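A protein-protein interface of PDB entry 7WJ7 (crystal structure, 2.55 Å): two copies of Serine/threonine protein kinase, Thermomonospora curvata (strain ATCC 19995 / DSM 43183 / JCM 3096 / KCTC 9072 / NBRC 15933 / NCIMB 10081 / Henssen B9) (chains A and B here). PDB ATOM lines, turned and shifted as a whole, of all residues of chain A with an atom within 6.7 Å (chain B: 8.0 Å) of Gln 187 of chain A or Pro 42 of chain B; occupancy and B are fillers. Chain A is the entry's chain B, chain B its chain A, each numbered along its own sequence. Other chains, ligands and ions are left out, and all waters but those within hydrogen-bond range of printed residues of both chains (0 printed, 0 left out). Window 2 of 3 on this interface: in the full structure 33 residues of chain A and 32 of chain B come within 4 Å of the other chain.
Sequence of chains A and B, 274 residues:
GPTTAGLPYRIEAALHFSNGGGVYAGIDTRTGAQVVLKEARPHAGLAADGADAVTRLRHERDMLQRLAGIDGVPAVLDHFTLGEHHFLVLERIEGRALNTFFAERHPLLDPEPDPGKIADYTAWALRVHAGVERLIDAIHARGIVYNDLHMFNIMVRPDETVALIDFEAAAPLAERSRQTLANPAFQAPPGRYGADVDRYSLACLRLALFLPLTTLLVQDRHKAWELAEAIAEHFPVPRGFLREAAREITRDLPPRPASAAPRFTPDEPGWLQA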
ATOM      1  N   THR A 180      13.656  22.518  14.933  1.00  0.00           N
ATOM      2  CA  THR A 180      14.309  22.355  16.254  1.00  0.00           C
ATOM      3  C   THR A 180      15.810  22.152  16.039  1.00  0.00           C
ATOM      4  O   THR A 180      16.184  21.229  15.300  1.00  0.00           O
ATOM      5  CB  THR A 180      13.729  21.152  16.999  1.00  0.00           C
ATOM      6  OG1 THR A 180      14.769  20.666  17.844  1.00  0.00           O
ATOM      7  CG2 THR A 180      13.242  20.066  16.064  1.00  0.00           C
ATOM      8  N   LEU A 181      16.631  22.996  16.654  1.00  0.00           N
ATOM      9  CA  LEU A 181      18.103  22.840  16.556  1.00  0.00           C
ATOM     10  C   LEU A 181      18.535  21.811  17.602  1.00  0.00           C
ATOM     11  O   LEU A 181      17.955  21.811  18.697  1.00  0.00           O
ATOM     12  CB  LEU A 181      18.765  24.202  16.787  1.00  0.00           C
ATOM     13  CG  LEU A 181      18.450  25.281  15.753  1.00  0.00           C
ATOM     14  CD1 LEU A 181      19.420  26.444  15.878  1.00  0.00           C
ATOM     15  CD2 LEU A 181      18.488  24.715  14.343  1.00  0.00           C
ATOM     16  N   ALA A 182      19.510  20.967  17.269  1.00  0.00           N
ATOM     17  CA  ALA A 182      19.907  19.889  18.202  1.00  0.00           C
ATOM     18  C   ALA A 182      20.899  20.389  19.241  1.00  0.00           C
ATOM     19  O   ALA A 182      21.564  21.407  19.003  1.00  0.00           O
ATOM     20  CB  ALA A 182      20.467  18.700  17.472  1.00  0.00           C
ATOM     21  N   ASN A 183      20.977  19.662  20.346  1.00  0.00           N
ATOM     22  CA  ASN A 183      21.919  20.024  21.424  1.00  0.00           C
ATOM     23  C   ASN A 183      23.094  19.062  21.298  1.00  0.00           C
ATOM     24  O   ASN A 183      22.869  17.930  20.862  1.00  0.00           O
ATOM     25  CB  ASN A 183      21.178  20.067  22.770  1.00  0.00           C
ATOM     26  CG  ASN A 183      21.803  19.258  23.883  1.00  0.00           C
ATOM     27  OD1 ASN A 183      21.428  18.113  24.095  1.00  0.00           O
ATOM     28  ND2 ASN A 183      22.710  19.863  24.630  1.00  0.00           N
ATOM     29  N   ALA A 185      24.356  17.098  23.226  1.00  0.00           N
ATOM     30  CA  ALA A 185      24.239  15.871  24.042  1.00  0.00           C
ATOM     31  C   ALA A 185      23.078  14.980  23.616  1.00  0.00           C
ATOM     32  O   ALA A 185      23.247  13.757  23.661  1.00  0.00           O
ATOM     33  CB  ALA A 185      24.038  16.291  25.464  1.00  0.00           C
ATOM     34  N   PHE A 186      21.944  15.563  23.244  1.00  0.00           N
ATOM     35  CA  PHE A 186      20.747  14.732  22.973  1.00  0.00           C
ATOM     36  C   PHE A 186      20.110  15.078  21.627  1.00  0.00           C
ATOM     37  O   PHE A 186      20.252  16.225  21.182  1.00  0.00           O
ATOM     38  CB  PHE A 186      19.752  14.864  24.129  1.00  0.00           C
ATOM     39  CG  PHE A 186      20.275  14.410  25.468  1.00  0.00           C
ATOM     40  CD1 PHE A 186      20.573  13.079  25.698  1.00  0.00           C
ATOM     41  CD2 PHE A 186      20.484  15.314  26.494  1.00  0.00           C
ATOM     42  CE1 PHE A 186      21.059  12.662  26.926  1.00  0.00           C
ATOM     43  CE2 PHE A 186      20.971  14.899  27.722  1.00  0.00           C
ATOM     44  CZ  PHE A 186      21.257  13.574  27.936  1.00  0.00           C
ATOM     45  N   GLN A 187      19.429  14.108  21.011  1.00  0.00           N
ATOM     46  CA  GLN A 187      18.748  14.297  19.739  1.00  0.00           C
ATOM     47  C   GLN A 187      17.759  15.454  19.831  1.00  0.00           C
ATOM     48  O   GLN A 187      17.173  15.716  20.885  1.00  0.00           O
ATOM     49  CB  GLN A 187      18.019  13.010  19.344  1.00  0.00           C
ATOM     50  CG  GLN A 187      17.293  13.051  18.009  1.00  0.00           C
ATOM     51  CD  GLN A 187      18.202  12.740  16.838  1.00  0.00           C
ATOM     52  OE1 GLN A 187      19.038  13.555  16.451  1.00  0.00           O
ATOM     53  NE2 GLN A 187      18.050  11.547  16.275  1.00  0.00           N
ATOM     54  N   ALA A 188      17.584  16.152  18.714  1.00  0.00           N
ATOM     55  CA  ALA A 188      16.652  17.270  18.670  1.00  0.00           C
ATOM     56  C   ALA A 188      15.235  16.780  18.958  1.00  0.00           C
ATOM     57  O   ALA A 188      14.798  15.780  18.370  1.00  0.00           O
ATOM     58  CB  ALA A 188      16.708  17.962  17.308  1.00  0.00           C
ATOM     59  N   PRO A 189      14.492  17.446  19.836  1.00  0.00           N
ATOM     60  CA  PRO A 189      13.165  16.950  20.223  1.00  0.00           C
ATOM     61  C   PRO A 189      12.161  17.153  19.105  1.00  0.00           C
ATOM     62  O   PRO A 189      12.117  18.222  18.479  1.00  0.00           O
ATOM     63  CB  PRO A 189      12.806  17.793  21.455  1.00  0.00           C
ATOM     64  CG  PRO A 189      13.720  18.965  21.433  1.00  0.00           C
ATOM     65  CD  PRO A 189      14.809  18.754  20.431  1.00  0.00           C
ATOM     66  N   PRO A 190      11.329  16.149  18.831  1.00  0.00           N
ATOM     67  CA  PRO A 190      10.404  16.244  17.694  1.00  0.00           C
ATOM     68  C   PRO A 190       9.219  17.145  18.013  1.00  0.00           C
ATOM     69  O   PRO A 190       8.529  16.958  19.017  1.00  0.00           O
ATOM     70  CB  PRO A 190       9.962  14.790  17.476  1.00  0.00           C
ATOM     71  CG  PRO A 190      10.884  13.947  18.327  1.00  0.00           C
ATOM     72  CD  PRO A 190      11.276  14.825  19.466  1.00  0.00           C
ATOM     73  N   TYR A 200      13.581  22.854  26.685  1.00  0.00           N
ATOM     74  CA  TYR A 200      14.230  21.571  26.438  1.00  0.00           C
ATOM     75  C   TYR A 200      15.741  21.682  26.594  1.00  0.00           C
ATOM     76  O   TYR A 200      16.368  20.845  27.252  1.00  0.00           O
ATOM     77  CB  TYR A 200      13.862  21.053  25.046  1.00  0.00           C
ATOM     78  CG  TYR A 200      14.533  19.747  24.674  1.00  0.00           C
ATOM     79  CD1 TYR A 200      15.793  19.724  24.080  1.00  0.00           C
ATOM     80  CD2 TYR A 200      13.923  18.534  24.956  1.00  0.00           C
ATOM     81  CE1 TYR A 200      16.401  18.527  23.744  1.00  0.00           C
ATOM     82  CE2 TYR A 200      14.527  17.336  24.635  1.00  0.00           C
ATOM     83  CZ  TYR A 200      15.766  17.336  24.032  1.00  0.00           C
ATOM     84  OH  TYR A 200      16.368  16.142  23.711  1.00  0.00           O
ATOM     85  N   CYS A 204      18.387  19.660  29.164  1.00  0.00           N
ATOM     86  CA  CYS A 204      19.612  18.999  28.725  1.00  0.00           C
ATOM     87  C   CYS A 204      20.827  19.556  29.456  1.00  0.00           C
ATOM     88  O   CYS A 204      21.727  18.802  29.844  1.00  0.00           O
ATOM     89  CB  CYS A 204      19.777  19.152  27.213  1.00  0.00           C
ATOM     90  SG  CYS A 204      18.556  18.249  26.243  1.00  0.00           S
ATOM     91  N   ASP A 220      22.006   8.376  24.805  1.00  0.00           N
ATOM     92  CA  ASP A 220      20.904   9.065  24.155  1.00  0.00           C
ATOM     93  C   ASP A 220      19.836   9.444  25.182  1.00  0.00           C
ATOM     94  O   ASP A 220      19.948   9.156  26.377  1.00  0.00           O
ATOM     95  CB  ASP A 220      20.331   8.199  23.034  1.00  0.00           C
ATOM     96  CG  ASP A 220      19.812   6.866  23.536  1.00  0.00           C
ATOM     97  OD1 ASP A 220      20.298   6.397  24.586  1.00  0.00           O
ATOM     98  OD2 ASP A 220      18.924   6.283  22.877  1.00  0.00           O
ATOM     99  N   ARG A 221      18.773  10.095  24.705  1.00  0.00           N
ATOM    100  CA  ARG A 221      17.783  10.713  25.580  1.00  0.00           C
ATOM    101  C   ARG A 221      16.809   9.720  26.205  1.00  0.00           C
ATOM    102  O   ARG A 221      16.108  10.089  27.155  1.00  0.00           O
ATOM    103  CB  ARG A 221      17.022  11.788  24.802  1.00  0.00           C
ATOM    104  CG  ARG A 221      16.092  11.245  23.742  1.00  0.00           C
ATOM    105  CD  ARG A 221      15.505  12.379  22.925  1.00  0.00           C
ATOM    106  NE  ARG A 221      14.286  12.905  23.522  1.00  0.00           N
ATOM    107  CZ  ARG A 221      13.214  13.261  22.828  1.00  0.00           C
ATOM    108  NH1 ARG A 221      13.180  13.155  21.510  1.00  0.00           N
ATOM    109  NH2 ARG A 221      12.149  13.727  23.473  1.00  0.00           N
ATOM    110  N   ILE A 249      12.997  16.055  29.134  1.00  0.00           N
ATOM    111  CA  ILE A 249      13.706  15.525  27.934  1.00  0.00           C
ATOM    112  C   ILE A 249      12.873  14.388  27.338  1.00  0.00           C
ATOM    113  O   ILE A 249      12.882  14.237  26.111  1.00  0.00           O
ATOM    114  CB  ILE A 249      15.147  15.120  28.301  1.00  0.00           C
ATOM    115  CG1 ILE A 249      16.010  16.346  28.595  1.00  0.00           C
ATOM    116  CG2 ILE A 249      15.792  14.238  27.247  1.00  0.00           C
ATOM    117  CD1 ILE A 249      17.231  16.029  29.412  1.00  0.00           C
ATOM    118  N   GLY B  20      24.799  21.713  14.083  1.00  0.00           N
ATOM    119  CA  GLY B  20      24.465  20.399  14.596  1.00  0.00           C
ATOM    120  C   GLY B  20      25.616  19.425  14.679  1.00  0.00           C
ATOM    121  O   GLY B  20      25.393  18.248  14.980  1.00  0.00           O
ATOM    122  N   GLU B  39      31.065  14.315  15.459  1.00  0.00           N
ATOM    123  CA  GLU B  39      29.819  13.578  15.583  1.00  0.00           C
ATOM    124  C   GLU B  39      28.678  14.376  14.969  1.00  0.00           C
ATOM    125  O   GLU B  39      28.747  15.601  14.829  1.00  0.00           O
ATOM    126  CB  GLU B  39      29.505  13.241  17.052  1.00  0.00           C
ATOM    127  CG  GLU B  39      29.529  14.429  18.003  1.00  0.00           C
ATOM    128  CD  GLU B  39      28.198  15.151  18.060  1.00  0.00           C
ATOM    129  OE1 GLU B  39      27.153  14.468  17.986  1.00  0.00           O
ATOM    130  OE2 GLU B  39      28.194  16.393  18.194  1.00  0.00           O
ATOM    131  N   ALA B  40      27.623  13.654  14.601  1.00  0.00           N
ATOM    132  CA  ALA B  40      26.458  14.254  13.970  1.00  0.00           C
ATOM    133  C   ALA B  40      25.252  13.361  14.220  1.00  0.00           C
ATOM    134  O   ALA B  40      25.359  12.133  14.161  1.00  0.00           O
ATOM    135  CB  ALA B  40      26.673  14.451  12.464  1.00  0.00           C
ATOM    136  N   ARG B  41      24.118  13.985  14.513  1.00  0.00           N
ATOM    137  CA  ARG B  41      22.857  13.288  14.665  1.00  0.00           C
ATOM    138  C   ARG B  41      21.938  13.629  13.497  1.00  0.00           C
ATOM    139  O   ARG B  41      21.964  14.761  13.005  1.00  0.00           O
ATOM    140  CB  ARG B  41      22.180  13.662  15.990  1.00  0.00           C
ATOM    141  CG  ARG B  41      22.473  12.688  17.127  1.00  0.00           C
ATOM    142  CD  ARG B  41      21.962  13.209  18.460  1.00  0.00           C
ATOM    143  NE  ARG B  41      23.002  13.222  19.483  1.00  0.00           N
ATOM    144  CZ  ARG B  41      23.676  14.303  19.854  1.00  0.00           C
ATOM    145  NH1 ARG B  41      23.448  15.483  19.302  1.00  0.00           N
ATOM    146  NH2 ARG B  41      24.603  14.196  20.803  1.00  0.00           N
ATOM    147  N   PRO B  42      21.141  12.675  13.015  1.00  0.00           N
ATOM    148  CA  PRO B  42      20.295  12.946  11.847  1.00  0.00           C
ATOM    149  C   PRO B  42      19.305  14.068  12.118  1.00  0.00           C
ATOM    150  O   PRO B  42      18.917  14.321  13.261  1.00  0.00           O
ATOM    151  CB  PRO B  42      19.584  11.610  11.604  1.00  0.00           C
ATOM    152  CG  PRO B  42      19.677  10.888  12.912  1.00  0.00           C
ATOM    153  CD  PRO B  42      20.996  11.291  13.488  1.00  0.00           C
ATOM    154  N   HIS B  43      18.918  14.755  11.038  1.00  0.00           N
ATOM    155  CA  HIS B  43      18.013  15.903  11.057  1.00  0.00           C
ATOM    156  C   HIS B  43      18.646  17.136  11.695  1.00  0.00           C
ATOM    157  O   HIS B  43      18.112  18.243  11.566  1.00  0.00           O
ATOM    158  CB  HIS B  43      16.700  15.560  11.773  1.00  0.00           C
ATOM    159  CG  HIS B  43      16.109  14.250  11.358  1.00  0.00           C
ATOM    160  ND1 HIS B  43      15.977  13.183  12.221  1.00  0.00           N
ATOM    161  CD2 HIS B  43      15.620  13.833  10.167  1.00  0.00           C
ATOM    162  CE1 HIS B  43      15.425  12.168  11.580  1.00  0.00           C
ATOM    163  NE2 HIS B  43      15.199  12.537  10.332  1.00  0.00           N
ATOM    164  N   ALA B  44      19.776  16.969  12.375  1.00  0.00           N
ATOM    165  CA  ALA B  44      20.433  18.103  13.007  1.00  0.00           C
ATOM    166  C   ALA B  44      21.140  18.957  11.967  1.00  0.00           C
ATOM    167  O   ALA B  44      21.777  18.441  11.045  1.00  0.00           O
ATOM    168  CB  ALA B  44      21.436  17.631  14.056  1.00  0.00           C
ATOM    169  N   GLY B  45      21.030  20.274  12.127  1.00  0.00           N
ATOM    170  CA  GLY B  45      21.707  21.190  11.233  1.00  0.00           C
ATOM    171  C   GLY B  45      21.142  21.240   9.835  1.00  0.00           C
ATOM    172  O   GLY B  45      21.850  21.640   8.907  1.00  0.00           O
ATOM    173  N   LEU B  46      19.882  20.842   9.660  1.00  0.00           N
ATOM    174  CA  LEU B  46      19.256  20.819   8.344  1.00  0.00           C
ATOM    175  C   LEU B  46      19.351  22.180   7.676  1.00  0.00           C
ATOM    176  O   LEU B  46      18.858  23.182   8.203  1.00  0.00           O
ATOM    177  CB  LEU B  46      17.792  20.392   8.467  1.00  0.00           C
ATOM    178  CG  LEU B  46      17.037  20.273   7.141  1.00  0.00           C
ATOM    179  CD1 LEU B  46      17.697  19.251   6.221  1.00  0.00           C
ATOM    180  CD2 LEU B  46      15.573  19.931   7.374  1.00  0.00           C
ATOM    181  N   ASP B  52      21.893  17.789   6.119  1.00  0.00           N
ATOM    182  CA  ASP B  52      21.995  17.848   7.566  1.00  0.00           C
ATOM    183  C   ASP B  52      23.440  17.557   7.982  1.00  0.00           C
ATOM    184  O   ASP B  52      24.337  17.431   7.142  1.00  0.00           O
ATOM    185  CB  ASP B  52      20.979  16.899   8.214  1.00  0.00           C
ATOM    186  CG  ASP B  52      21.256  15.433   7.922  1.00  0.00           C
ATOM    187  OD1 ASP B  52      22.176  15.124   7.134  1.00  0.00           O
ATOM    188  OD2 ASP B  52      20.547  14.580   8.498  1.00  0.00           O
ATOM    189  N   ALA B  53      23.675  17.453   9.292  1.00  0.00           N
ATOM    190  CA  ALA B  53      25.040  17.293   9.786  1.00  0.00           C
ATOM    191  C   ALA B  53      25.611  15.920   9.453  1.00  0.00           C
ATOM    192  O   ALA B  53      26.830  15.781   9.296  1.00  0.00           O
ATOM    193  CB  ALA B  53      25.089  17.540  11.293  1.00  0.00           C
ATOM    194  N   VAL B  54      24.759  14.898   9.355  1.00  0.00           N
ATOM    195  CA  VAL B  54      25.228  13.594   8.899  1.00  0.00           C
ATOM    196  C   VAL B  54      25.652  13.668   7.437  1.00  0.00           C
ATOM    197  O   VAL B  54      26.687  13.116   7.046  1.00  0.00           O
ATOM    198  CB  VAL B  54      24.139  12.527   9.123  1.00  0.00           C
ATOM    199  CG1 VAL B  54      24.394  11.302   8.253  1.00  0.00           C
ATOM    200  CG2 VAL B  54      24.075  12.135  10.591  1.00  0.00           C
ATOM    201  N   THR B  55      24.865  14.362   6.610  1.00  0.00           N
ATOM    202  CA  THR B  55      25.217  14.534   5.205  1.00  0.00           C
ATOM    203  C   THR B  55      26.578  15.206   5.059  1.00  0.00           C
ATOM    204  O   THR B  55      27.442  14.732   4.309  1.00  0.00           O
ATOM    205  CB  THR B  55      24.138  15.349   4.490  1.00  0.00           C
ATOM    206  OG1 THR B  55      22.970  14.541   4.301  1.00  0.00           O
ATOM    207  CG2 THR B  55      24.641  15.831   3.140  1.00  0.00           C
ATOM    208  N   LEU B  82      26.325   4.815  16.547  1.00  0.00           N
ATOM    209  CA  LEU B  82      25.824   4.363  17.850  1.00  0.00           C
ATOM    210  C   LEU B  82      24.343   4.737  17.894  1.00  0.00           C
ATOM    211  O   LEU B  82      23.977   5.820  18.355  1.00  0.00           O
ATOM    212  CB  LEU B  82      26.607   4.989  18.996  1.00  0.00           C
ATOM    213  CG  LEU B  82      28.062   4.568  19.205  1.00  0.00           C
ATOM    214  CD1 LEU B  82      28.527   5.023  20.573  1.00  0.00           C
ATOM    215  CD2 LEU B  82      28.234   3.061  19.068  1.00  0.00           C
ATOM    216  N   GLY B  83      23.499   3.830  17.420  1.00  0.00           N
ATOM    217  CA  GLY B  83      22.116   4.187  17.147  1.00  0.00           C
ATOM    218  C   GLY B  83      22.041   4.841  15.786  1.00  0.00           C
ATOM    219  O   GLY B  83      22.509   4.279  14.792  1.00  0.00           O
ATOM    220  N   GLU B  84      21.460   6.035  15.730  1.00  0.00           N
ATOM    221  CA  GLU B  84      21.551   6.881  14.547  1.00  0.00           C
ATOM    222  C   GLU B  84      22.698   7.879  14.649  1.00  0.00           C
ATOM    223  O   GLU B  84      22.833   8.749  13.782  1.00  0.00           O
ATOM    224  CB  GLU B  84      20.228   7.617  14.320  1.00  0.00           C
ATOM    225  N   HIS B  85      23.532   7.750  15.678  1.00  0.00           N
ATOM    226  CA  HIS B  85      24.580   8.712  15.991  1.00  0.00           C
ATOM    227  C   HIS B  85      25.853   8.358  15.230  1.00  0.00           C
ATOM    228  O   HIS B  85      26.443   7.301  15.466  1.00  0.00           O
ATOM    229  CB  HIS B  85      24.840   8.707  17.497  1.00  0.00           C
ATOM    230  CG  HIS B  85      25.412   9.984  18.021  1.00  0.00           C
ATOM    231  ND1 HIS B  85      25.561  10.228  19.369  1.00  0.00           N
ATOM    232  CD2 HIS B  85      25.877  11.085  17.385  1.00  0.00           C
ATOM    233  CE1 HIS B  85      26.091  11.427  19.541  1.00  0.00           C
ATOM    234  NE2 HIS B  85      26.293  11.966  18.353  1.00  0.00           N
ATOM    235  N   HIS B  86      26.289   9.249  14.344  1.00  0.00           N
ATOM    236  CA  HIS B  86      27.478   9.028  13.532  1.00  0.00           C
ATOM    237  C   HIS B  86      28.703   9.654  14.188  1.00  0.00           C
ATOM    238  O   HIS B  86      28.634  10.760  14.730  1.00  0.00           O
ATOM    239  CB  HIS B  86      27.294   9.609  12.128  1.00  0.00           C
ATOM    240  CG  HIS B  86      26.267   8.898  11.304  1.00  0.00           C
ATOM    241  ND1 HIS B  86      24.947   8.792  11.686  1.00  0.00           N
ATOM    242  CD2 HIS B  86      26.366   8.263  10.113  1.00  0.00           C
ATOM    243  CE1 HIS B  86      24.277   8.119  10.767  1.00  0.00           C
ATOM    244  NE2 HIS B  86      25.114   7.787   9.802  1.00  0.00           N
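Of the printed residues of chain B, Asn 183 of chain A touches Arg 41. Printed residues of chain B within 4 Å of Ala 185 of chain A: Arg 41. Of the printed residues of chain B, Gln 187 of chain A touches Arg 41 and Pro 42. Ala 188 of chain A touches none of the printed residues of chain B. Pro 42 of chain B touches just one residue of chain A: Gln 187. Printed residues of chain A within 4 Å of Ala 44 of chain B: Ala 182. Ala 53 of chain B touches none of the printed residues of chain A. The nearest residue of chain B that does not touch Gln 187 of chain A is His 43 of chain B (4.8 Å). The nearest residue of chain A that does not touch Pro 42 of chain B is Ala 188 of chain A (5.9 Å).
Of the 15 printed residues of chain A, 5 touch a printed residue of chain B. Printed residues of chain A that touch a printed residue of chain B: Ala 182, Asn 183, Ala 185, Phe 186 and Gln 187. Hydrophobic or aromatic side chains of chain A within 4 Å of the printed part of chain B: Ala 182. Among the printed residues, 6 pairs touch across the chains. Among the printed residues, no Asp or Glu carboxylate lies within 4 Å of a Lys or Arg side-chain nitrogen of the other chain.
No position is printed for both chains.
CB of Ala 182 of chain A touches CB of Ala 44 of chain B (3.7 Å). Phe 186 of chain A touches Arg 41 of chain B. Arg 41 of chain B touches Gln 187 of chain A.
The side-chain carboxylate of Glu 39 of chain B lies within salt-bridge range of the guanidinium group of Arg 41 of chain B, 3.8 Å away. The backbone NH (N) of Ala 53 of chain B lies within hydrogen-bond range of the backbone carbonyl oxygen (O) of Ala 44 of chain B. The side-chain amide oxygen of Asn 183 of chain A lies close to the backbone NH of Ala 185 of chain A (3.2 Å). OD1 of Asn 183 of chain A is in hydrogen-bond range of N of Phe 186 of chain A. OD1 of Asn 183 of chain A is in hydrogen-bond range of SG of Cys 204 of chain A, 3.6 Å away. O of Gln 187 of chain A sits at hydrogen-bond distance from OH of Tyr 200 of chain A.
The guanidinium group (NH1) of Arg 41 of chain B lies within hydrogen-bond range of the backbone carbonyl oxygen (O) of Asn 183 of chain A (3.0 Å). O of Ala 185 of chain A is in hydrogen-bond range of NH2 of Arg 41 of chain B (3.2 Å). O of Pro 42 of chain B sits close to OE1 of Gln 187 of chain A (3.3 Å).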
